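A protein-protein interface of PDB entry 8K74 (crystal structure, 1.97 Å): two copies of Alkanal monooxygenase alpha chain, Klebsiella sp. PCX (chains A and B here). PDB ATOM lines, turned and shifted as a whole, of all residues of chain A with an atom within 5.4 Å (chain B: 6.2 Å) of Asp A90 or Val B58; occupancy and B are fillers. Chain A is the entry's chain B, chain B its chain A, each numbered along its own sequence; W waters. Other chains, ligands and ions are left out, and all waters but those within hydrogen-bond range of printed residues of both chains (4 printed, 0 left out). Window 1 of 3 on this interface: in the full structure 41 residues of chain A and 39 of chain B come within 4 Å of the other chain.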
ATOM      1  N   LEU A  57       0.490  11.395 -33.961  1.00  0.00           N
ATOM      2  CA  LEU A  57       1.305  12.536 -33.547  1.00  0.00           C
ATOM      3  C   LEU A  57       2.756  12.133 -33.330  1.00  0.00           C
ATOM      4  O   LEU A  57       3.667  12.945 -33.545  1.00  0.00           O
ATOM      5  CB  LEU A  57       0.720  13.166 -32.277  1.00  0.00           C
ATOM      6  CG  LEU A  57      -0.722  13.668 -32.496  1.00  0.00           C
ATOM      7  CD1 LEU A  57      -1.299  14.251 -31.238  1.00  0.00           C
ATOM      8  CD2 LEU A  57      -0.847  14.674 -33.618  1.00  0.00           C
ATOM      9  N   VAL A  58       2.987  10.893 -32.903  1.00  0.00           N
ATOM     10  CA  VAL A  58       4.346  10.395 -32.749  1.00  0.00           C
ATOM     11  C   VAL A  58       4.989  10.186 -34.118  1.00  0.00           C
ATOM     12  O   VAL A  58       6.136  10.593 -34.362  1.00  0.00           O
ATOM     13  CB  VAL A  58       4.325   9.105 -31.905  1.00  0.00           C
ATOM     14  CG1 VAL A  58       5.680   8.434 -31.890  1.00  0.00           C
ATOM     15  CG2 VAL A  58       3.868   9.428 -30.467  1.00  0.00           C
ATOM     16  N   ALA A  61       5.877  13.522 -35.843  1.00  0.00           N
ATOM     17  CA  ALA A  61       7.097  14.105 -35.288  1.00  0.00           C
ATOM     18  C   ALA A  61       8.335  13.524 -35.960  1.00  0.00           C
ATOM     19  O   ALA A  61       9.290  14.250 -36.260  1.00  0.00           O
ATOM     20  CB  ALA A  61       7.157  13.869 -33.776  1.00  0.00           C
ATOM     21  N   LEU A  85      -6.901  16.085 -23.217  1.00  0.00           N
ATOM     22  CA  LEU A  85      -5.864  17.027 -22.797  1.00  0.00           C
ATOM     23  C   LEU A  85      -4.487  16.586 -23.273  1.00  0.00           C
ATOM     24  O   LEU A  85      -3.661  17.426 -23.657  1.00  0.00           O
ATOM     25  CB  LEU A  85      -5.879  17.196 -21.284  1.00  0.00           C
ATOM     26  CG  LEU A  85      -4.947  18.260 -20.701  1.00  0.00           C
ATOM     27  CD1 LEU A  85      -5.058  19.631 -21.408  1.00  0.00           C
ATOM     28  CD2 LEU A  85      -5.233  18.405 -19.229  1.00  0.00           C
ATOM     29  N   ARG A  86      -4.218  15.274 -23.247  1.00  0.00           N
ATOM     30  CA  ARG A  86      -2.950  14.789 -23.776  1.00  0.00           C
ATOM     31  C   ARG A  86      -2.868  15.010 -25.283  1.00  0.00           C
ATOM     32  O   ARG A  86      -1.803  15.362 -25.809  1.00  0.00           O
ATOM     33  CB  ARG A  86      -2.749  13.310 -23.395  1.00  0.00           C
ATOM     34  CG  ARG A  86      -2.632  13.098 -21.846  1.00  0.00           C
ATOM     35  CD  ARG A  86      -1.249  13.572 -21.365  1.00  0.00           C
ATOM     36  NE  ARG A  86      -0.209  12.898 -22.130  1.00  0.00           N
ATOM     37  CZ  ARG A  86       0.599  13.504 -22.988  1.00  0.00           C
ATOM     38  NH1 ARG A  86       0.527  14.810 -23.203  1.00  0.00           N
ATOM     39  NH2 ARG A  86       1.434  12.770 -23.718  1.00  0.00           N
ATOM     40  N   VAL A  87      -3.981  14.837 -26.004  1.00  0.00           N
ATOM     41  CA  VAL A  87      -3.974  15.188 -27.425  1.00  0.00           C
ATOM     42  C   VAL A  87      -3.630  16.663 -27.604  1.00  0.00           C
ATOM     43  O   VAL A  87      -2.825  17.041 -28.472  1.00  0.00           O
ATOM     44  CB  VAL A  87      -5.328  14.864 -28.071  1.00  0.00           C
ATOM     45  CG1 VAL A  87      -5.338  15.371 -29.515  1.00  0.00           C
ATOM     46  CG2 VAL A  87      -5.605  13.387 -28.005  1.00  0.00           C
ATOM     47  N   ALA A  88      -4.260  17.521 -26.801  1.00  0.00           N
ATOM     48  CA  ALA A  88      -3.986  18.951 -26.883  1.00  0.00           C
ATOM     49  C   ALA A  88      -2.499  19.234 -26.706  1.00  0.00           C
ATOM     50  O   ALA A  88      -1.920  20.005 -27.475  1.00  0.00           O
ATOM     51  CB  ALA A  88      -4.808  19.717 -25.838  1.00  0.00           C
ATOM     52  N   GLU A  89      -1.870  18.616 -25.690  1.00  0.00           N
ATOM     53  CA  GLU A  89      -0.445  18.814 -25.434  1.00  0.00           C
ATOM     54  C   GLU A  89       0.404  18.273 -26.579  1.00  0.00           C
ATOM     55  O   GLU A  89       1.281  18.970 -27.104  1.00  0.00           O
ATOM     56  CB  GLU A  89      -0.044  18.129 -24.115  1.00  0.00           C
ATOM     57  CG  GLU A  89      -0.602  18.838 -22.847  1.00  0.00           C
ATOM     58  CD  GLU A  89      -0.315  18.076 -21.563  1.00  0.00           C
ATOM     59  OE1 GLU A  89      -0.314  16.821 -21.605  1.00  0.00           O
ATOM     60  OE2 GLU A  89      -0.061  18.733 -20.521  1.00  0.00           O
ATOM     61  N   ASP A  90       0.172  17.014 -26.962  1.00  0.00           N
ATOM     62  CA  ASP A  90       0.956  16.408 -28.034  1.00  0.00           C
ATOM     63  C   ASP A  90       0.892  17.233 -29.313  1.00  0.00           C
ATOM     64  O   ASP A  90       1.919  17.448 -29.975  1.00  0.00           O
ATOM     65  CB  ASP A  90       0.485  14.974 -28.309  1.00  0.00           C
ATOM     66  CG  ASP A  90       0.918  13.978 -27.229  1.00  0.00           C
ATOM     67  OD1 ASP A  90       1.601  14.354 -26.244  1.00  0.00           O
ATOM     68  OD2 ASP A  90       0.653  12.777 -27.429  1.00  0.00           O
ATOM     69  N   ALA A  91      -0.309  17.694 -29.693  1.00  0.00           N
ATOM     70  CA  ALA A  91      -0.418  18.521 -30.900  1.00  0.00           C
ATOM     71  C   ALA A  91       0.267  19.875 -30.721  1.00  0.00           C
ATOM     72  O   ALA A  91       0.917  20.374 -31.649  1.00  0.00           O
ATOM     73  CB  ALA A  91      -1.889  18.716 -31.294  1.00  0.00           C
ATOM     74  N   ALA A  92       0.116  20.496 -29.544  1.00  0.00           N
ATOM     75  CA  ALA A  92       0.830  21.746 -29.266  1.00  0.00           C
ATOM     76  C   ALA A  92       2.339  21.575 -29.420  1.00  0.00           C
ATOM     77  O   ALA A  92       3.018  22.436 -30.004  1.00  0.00           O
ATOM     78  CB  ALA A  92       0.500  22.241 -27.856  1.00  0.00           C
ATOM     79  N   VAL A  93       2.885  20.475 -28.904  1.00  0.00           N
ATOM     80  CA  VAL A  93       4.318  20.238 -29.049  1.00  0.00           C
ATOM     81  C   VAL A  93       4.660  19.948 -30.503  1.00  0.00           C
ATOM     82  O   VAL A  93       5.612  20.514 -31.057  1.00  0.00           O
ATOM     83  CB  VAL A  93       4.780  19.094 -28.123  1.00  0.00           C
ATOM     84  CG1 VAL A  93       6.196  18.655 -28.484  1.00  0.00           C
ATOM     85  CG2 VAL A  93       4.694  19.499 -26.649  1.00  0.00           C
ATOM     86  N   LEU A  94       3.910  19.036 -31.131  1.00  0.00           N
ATOM     87  CA  LEU A  94       4.199  18.646 -32.511  1.00  0.00           C
ATOM     88  C   LEU A  94       4.244  19.852 -33.459  1.00  0.00           C
ATOM     89  O   LEU A  94       5.153  19.961 -34.295  1.00  0.00           O
ATOM     90  CB  LEU A  94       3.153  17.628 -32.990  1.00  0.00           C
ATOM     91  CG  LEU A  94       3.275  17.226 -34.458  1.00  0.00           C
ATOM     92  CD1 LEU A  94       4.689  16.736 -34.745  1.00  0.00           C
ATOM     93  CD2 LEU A  94       2.250  16.144 -34.806  1.00  0.00           C
ATOM     94  N   ASP A  95       3.279  20.768 -33.355  1.00  0.00           N
ATOM     95  CA  ASP A  95       3.259  21.874 -34.306  1.00  0.00           C
ATOM     96  C   ASP A  95       4.541  22.692 -34.217  1.00  0.00           C
ATOM     97  O   ASP A  95       5.100  23.106 -35.241  1.00  0.00           O
ATOM     98  CB  ASP A  95       2.046  22.769 -34.083  1.00  0.00           C
ATOM     99  CG  ASP A  95       1.929  23.848 -35.163  1.00  0.00           C
ATOM    100  OD1 ASP A  95       2.046  23.504 -36.352  1.00  0.00           O
ATOM    101  OD2 ASP A  95       1.678  25.030 -34.859  1.00  0.00           O
ATOM    102  N   LEU A  97       7.473  21.463 -33.295  1.00  0.00           N
ATOM    103  CA  LEU A  97       8.541  20.662 -33.899  1.00  0.00           C
ATOM    104  C   LEU A  97       8.480  20.655 -35.420  1.00  0.00           C
ATOM    105  O   LEU A  97       9.518  20.486 -36.078  1.00  0.00           O
ATOM    106  CB  LEU A  97       8.512  19.216 -33.391  1.00  0.00           C
ATOM    107  CG  LEU A  97       8.501  19.014 -31.880  1.00  0.00           C
ATOM    108  CD1 LEU A  97       8.348  17.522 -31.517  1.00  0.00           C
ATOM    109  CD2 LEU A  97       9.760  19.604 -31.305  1.00  0.00           C
ATOM    110  N   PRO B  54       5.505  18.384 -22.112  1.00  0.00           N
ATOM    111  CA  PRO B  54       4.486  17.424 -21.678  1.00  0.00           C
ATOM    112  C   PRO B  54       4.392  16.171 -22.531  1.00  0.00           C
ATOM    113  O   PRO B  54       3.579  15.302 -22.208  1.00  0.00           O
ATOM    114  CB  PRO B  54       3.192  18.253 -21.802  1.00  0.00           C
ATOM    115  CG  PRO B  54       3.458  19.137 -22.979  1.00  0.00           C
ATOM    116  CD  PRO B  54       4.928  19.505 -22.877  1.00  0.00           C
ATOM    117  N   SER B  55       5.159  16.060 -23.618  1.00  0.00           N
ATOM    118  CA  SER B  55       4.961  15.006 -24.621  1.00  0.00           C
ATOM    119  C   SER B  55       6.276  14.352 -24.988  1.00  0.00           C
ATOM    120  O   SER B  55       6.762  14.481 -26.125  1.00  0.00           O
ATOM    121  CB  SER B  55       4.272  15.560 -25.869  1.00  0.00           C
ATOM    122  OG  SER B  55       3.174  16.368 -25.466  1.00  0.00           O
ATOM    123  N   PRO B  56       6.862  13.604 -24.055  1.00  0.00           N
ATOM    124  CA  PRO B  56       8.191  13.020 -24.313  1.00  0.00           C
ATOM    125  C   PRO B  56       8.216  12.041 -25.480  1.00  0.00           C
ATOM    126  O   PRO B  56       9.228  11.981 -26.191  1.00  0.00           O
ATOM    127  CB  PRO B  56       8.524  12.314 -22.989  1.00  0.00           C
ATOM    128  CG  PRO B  56       7.137  11.970 -22.387  1.00  0.00           C
ATOM    129  CD  PRO B  56       6.302  13.201 -22.742  1.00  0.00           C
ATOM    130  N   LEU B  57       7.143  11.271 -25.698  1.00  0.00           N
ATOM    131  CA  LEU B  57       7.142  10.300 -26.792  1.00  0.00           C
ATOM    132  C   LEU B  57       7.121  10.982 -28.152  1.00  0.00           C
ATOM    133  O   LEU B  57       7.723  10.479 -29.114  1.00  0.00           O
ATOM    134  CB  LEU B  57       5.945   9.348 -26.659  1.00  0.00           C
ATOM    135  CG  LEU B  57       5.976   8.499 -25.380  1.00  0.00           C
ATOM    136  CD1 LEU B  57       4.788   7.536 -25.263  1.00  0.00           C
ATOM    137  CD2 LEU B  57       7.299   7.726 -25.265  1.00  0.00           C
ATOM    138  N   VAL B  58       6.440  12.123 -28.246  1.00  0.00           N
ATOM    139  CA  VAL B  58       6.431  12.898 -29.484  1.00  0.00           C
ATOM    140  C   VAL B  58       7.809  13.499 -29.744  1.00  0.00           C
ATOM    141  O   VAL B  58       8.344  13.428 -30.861  1.00  0.00           O
ATOM    142  CB  VAL B  58       5.332  13.974 -29.397  1.00  0.00           C
ATOM    143  CG1 VAL B  58       5.401  14.973 -30.577  1.00  0.00           C
ATOM    144  CG2 VAL B  58       3.959  13.291 -29.325  1.00  0.00           C
ATOM    145  N   PHE B  59       8.402  14.111 -28.715  1.00  0.00           N
ATOM    146  CA  PHE B  59       9.699  14.757 -28.892  1.00  0.00           C
ATOM    147  C   PHE B  59      10.787  13.730 -29.218  1.00  0.00           C
ATOM    148  O   PHE B  59      11.665  13.981 -30.055  1.00  0.00           O
ATOM    149  CB  PHE B  59      10.035  15.557 -27.630  1.00  0.00           C
ATOM    150  CG  PHE B  59      11.424  16.113 -27.624  1.00  0.00           C
ATOM    151  CD1 PHE B  59      11.688  17.334 -28.231  1.00  0.00           C
ATOM    152  CD2 PHE B  59      12.453  15.440 -27.010  1.00  0.00           C
ATOM    153  CE1 PHE B  59      12.982  17.847 -28.251  1.00  0.00           C
ATOM    154  CE2 PHE B  59      13.752  15.956 -27.011  1.00  0.00           C
ATOM    155  CZ  PHE B  59      14.009  17.146 -27.628  1.00  0.00           C
ATOM    156  N   LEU B  60      10.733  12.558 -28.576  1.00  0.00           N
ATOM    157  CA  LEU B  60      11.720  11.517 -28.846  1.00  0.00           C
ATOM    158  C   LEU B  60      11.601  10.960 -30.264  1.00  0.00           C
ATOM    159  O   LEU B  60      12.617  10.579 -30.866  1.00  0.00           O
ATOM    160  CB  LEU B  60      11.591  10.389 -27.818  1.00  0.00           C
ATOM    161  CG  LEU B  60      12.146  10.712 -26.427  1.00  0.00           C
ATOM    162  CD1 LEU B  60      12.065   9.481 -25.515  1.00  0.00           C
ATOM    163  CD2 LEU B  60      13.571  11.307 -26.485  1.00  0.00           C
ATOM    164  N   ALA B  61      10.382  10.891 -30.810  1.00  0.00           N
ATOM    165  CA  ALA B  61      10.247  10.476 -32.206  1.00  0.00           C
ATOM    166  C   ALA B  61      10.978  11.434 -33.128  1.00  0.00           C
ATOM    167  O   ALA B  61      11.553  11.012 -34.139  1.00  0.00           O
ATOM    168  CB  ALA B  61       8.774  10.398 -32.600  1.00  0.00           C
ATOM    169  N   HIS B  62      10.995  12.720 -32.775  1.00  0.00           N
ATOM    170  CA  HIS B  62      11.594  13.738 -33.628  1.00  0.00           C
ATOM    171  C   HIS B  62      13.120  13.693 -33.523  1.00  0.00           C
ATOM    172  O   HIS B  62      13.822  13.676 -34.541  1.00  0.00           O
ATOM    173  CB  HIS B  62      11.021  15.094 -33.221  1.00  0.00           C
ATOM    174  CG  HIS B  62      11.451  16.245 -34.081  1.00  0.00           C
ATOM    175  ND1 HIS B  62      12.590  16.979 -33.848  1.00  0.00           N
ATOM    176  CD2 HIS B  62      10.858  16.799 -35.171  1.00  0.00           C
ATOM    177  CE1 HIS B  62      12.687  17.934 -34.758  1.00  0.00           C
ATOM    178  NE2 HIS B  62      11.652  17.844 -35.575  1.00  0.00           N
ATOM    179  N   VAL B  63      13.654  13.576 -32.302  1.00  0.00           N
ATOM    180  CA  VAL B  63      15.116  13.502 -32.182  1.00  0.00           C
ATOM    181  C   VAL B  63      15.636  12.139 -32.644  1.00  0.00           C
ATOM    182  O   VAL B  63      16.785  12.020 -33.090  1.00  0.00           O
ATOM    183  CB  VAL B  63      15.553  13.830 -30.740  1.00  0.00           C
ATOM    184  CG1 VAL B  63      14.868  12.932 -29.772  1.00  0.00           C
ATOM    185  CG2 VAL B  63      17.075  13.742 -30.581  1.00  0.00           C
ATOM    186  N   ARG B  86      -3.104   4.448 -24.576  1.00  0.00           N
ATOM    187  CA  ARG B  86      -2.498   5.330 -25.562  1.00  0.00           C
ATOM    188  C   ARG B  86      -0.991   5.440 -25.329  1.00  0.00           C
ATOM    189  O   ARG B  86      -0.213   5.499 -26.289  1.00  0.00           O
ATOM    190  CB  ARG B  86      -3.188   6.708 -25.525  1.00  0.00           C
ATOM    191  CG  ARG B  86      -4.642   6.728 -26.084  1.00  0.00           C
ATOM    192  CD  ARG B  86      -4.664   6.300 -27.558  1.00  0.00           C
ATOM    193  NE  ARG B  86      -4.038   7.339 -28.366  1.00  0.00           N
ATOM    194  CZ  ARG B  86      -2.861   7.192 -28.957  1.00  0.00           C
ATOM    195  NH1 ARG B  86      -2.203   6.033 -28.912  1.00  0.00           N
ATOM    196  NH2 ARG B  86      -2.292   8.246 -29.538  1.00  0.00           N
ATOM    197  N   ASP B  90       1.665   4.534 -28.173  1.00  0.00           N
ATOM    198  CA  ASP B  90       2.702   5.468 -28.604  1.00  0.00           C
ATOM    199  C   ASP B  90       4.103   4.900 -28.389  1.00  0.00           C
ATOM    200  O   ASP B  90       4.995   5.108 -29.223  1.00  0.00           O
ATOM    201  CB  ASP B  90       2.580   6.813 -27.881  1.00  0.00           C
ATOM    202  CG  ASP B  90       1.346   7.622 -28.306  1.00  0.00           C
ATOM    203  OD1 ASP B  90       0.602   7.208 -29.212  1.00  0.00           O
ATOM    204  OD2 ASP B  90       1.178   8.739 -27.798  1.00  0.00           O
ATOM    205  N   LEU B  94       6.892   4.198 -31.163  1.00  0.00           N
ATOM    206  CA  LEU B  94       8.158   4.915 -31.038  1.00  0.00           C
ATOM    207  C   LEU B  94       9.350   3.965 -31.055  1.00  0.00           C
ATOM    208  O   LEU B  94      10.365   4.243 -31.707  1.00  0.00           O
ATOM    209  CB  LEU B  94       8.170   5.738 -29.750  1.00  0.00           C
ATOM    210  CG  LEU B  94       9.504   6.405 -29.409  1.00  0.00           C
ATOM    211  CD1 LEU B  94       9.904   7.306 -30.573  1.00  0.00           C
ATOM    212  CD2 LEU B  94       9.349   7.205 -28.126  1.00  0.00           C
HETATM  213  O   HOH W   1       4.509  11.607 -24.803  1.00  0.00           O
HETATM  214  O   HOH W   2      -0.920  10.208 -31.807  1.00  0.00           O
HETATM  215  O   HOH W   3       0.494  10.883 -29.380  1.00  0.00           O
HETATM  216  O   HOH W   4       2.464  10.878 -26.603  1.00  0.00           O
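NH1 of Arg A86 sits at hydrogen-bond distance from O of Pro B54, 3.2 Å away.
OG of Ser B55 sits at hydrogen-bond distance from OD1 of Asp A90 (2.7 Å).
NE2 of His B62 sits at hydrogen-bond distance from O of Leu A97 (3.4 Å).
Among the printed residues, pairs that only touch across the chains: Ala A61 with Val B58, Val A58 with Ala B61, Ala A61 with His B62, Glu A89 with Pro B54, Glu A89 with Ser B55, Val A93 with Ser B55, Asp A90 with Val B58, Val A93 with Pro B54, Val A58 with Asp B90, Arg A86 with Ser B55 and Leu A57 with Val B58.
Printed residues of chain A that touch a printed residue of chain B: Leu A57, Val A58, Ala A61, Arg A86, Glu A89, Asp A90, Val A93 and Leu A97.
Among the printed residues, 14 pairs touch across the chains.
Among the printed residues, no Asp or Glu carboxylate lies within 4 Å of a Lys or Arg side-chain nitrogen of the other chain.
Leu A57 touches Val B58, but with the chains exchanged Val A58 does not touch Leu B57 (4.01 Å).
Val A58 touches Ala B61, and with the chains exchanged Ala A61 touches Val B58.
Val A58 touches Asp B90, and with the chains exchanged Asp A90 touches Val B58.
6 positions are printed for both chains.
Of the 14 pairs that touch across the chains among the printed residues, 4 have their exchanged pair printed and touching as well.
Of the printed residues of chain B, Val A58 touches Ala B61 and Asp B90.
Of the printed residues of chain B, Ala A61 touches Val B58 and His B62.
Printed residues of chain B within 4 Å of Arg A86: Pro B54 (3.2 Å) and Ser B55 (3.8 Å).
Asp A90 touches two residues of chain B.
Of the printed residues of chain B, Val A93 touches Pro B54 and Ser B55.
Leu A94 touches none of the printed residues of chain B.
Of the printed residues of chain A, Val B58 touches Leu A57 (3.99 Å), Ala A61 (3.2 Å) and Asp A90 (3.8 Å).
Val B63 touches none of the printed residues of chain A.
Printed residues of chain A within 4 Å of Asp B90: Val A58 (3.8 Å).
Water W3 lies within hydrogen-bond range of OD2 of Asp A90 (2.7 Å) and OD2 of Asp B90 (2.8 Å).
Water W4 bridges the side-chain carboxylate of Asp A90 (2.8 Å) and the side-chain carboxylate of Asp B90 (2.8 Å).
Water W1 lies within hydrogen-bond range of N of Leu B57 and NH2 of Arg A86.
Water W2 bridges the backbone NH (N) of Leu A57 (2.8 Å) and the guanidinium group (NH2) of Arg B86 (3.3 Å).
OD1 of Asp B90 is in salt-bridge range of NH1 of Arg B86 (3.1 Å).
The guanidinium group (NH1) of Arg A86 is in salt-bridge range of the side-chain carboxylate (OE1) of Glu A89 (2.7 Å).
The side-chain carboxylate of Asp A90 is in salt-bridge range of the guanidinium group of Arg A86, at 3.0 Å.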
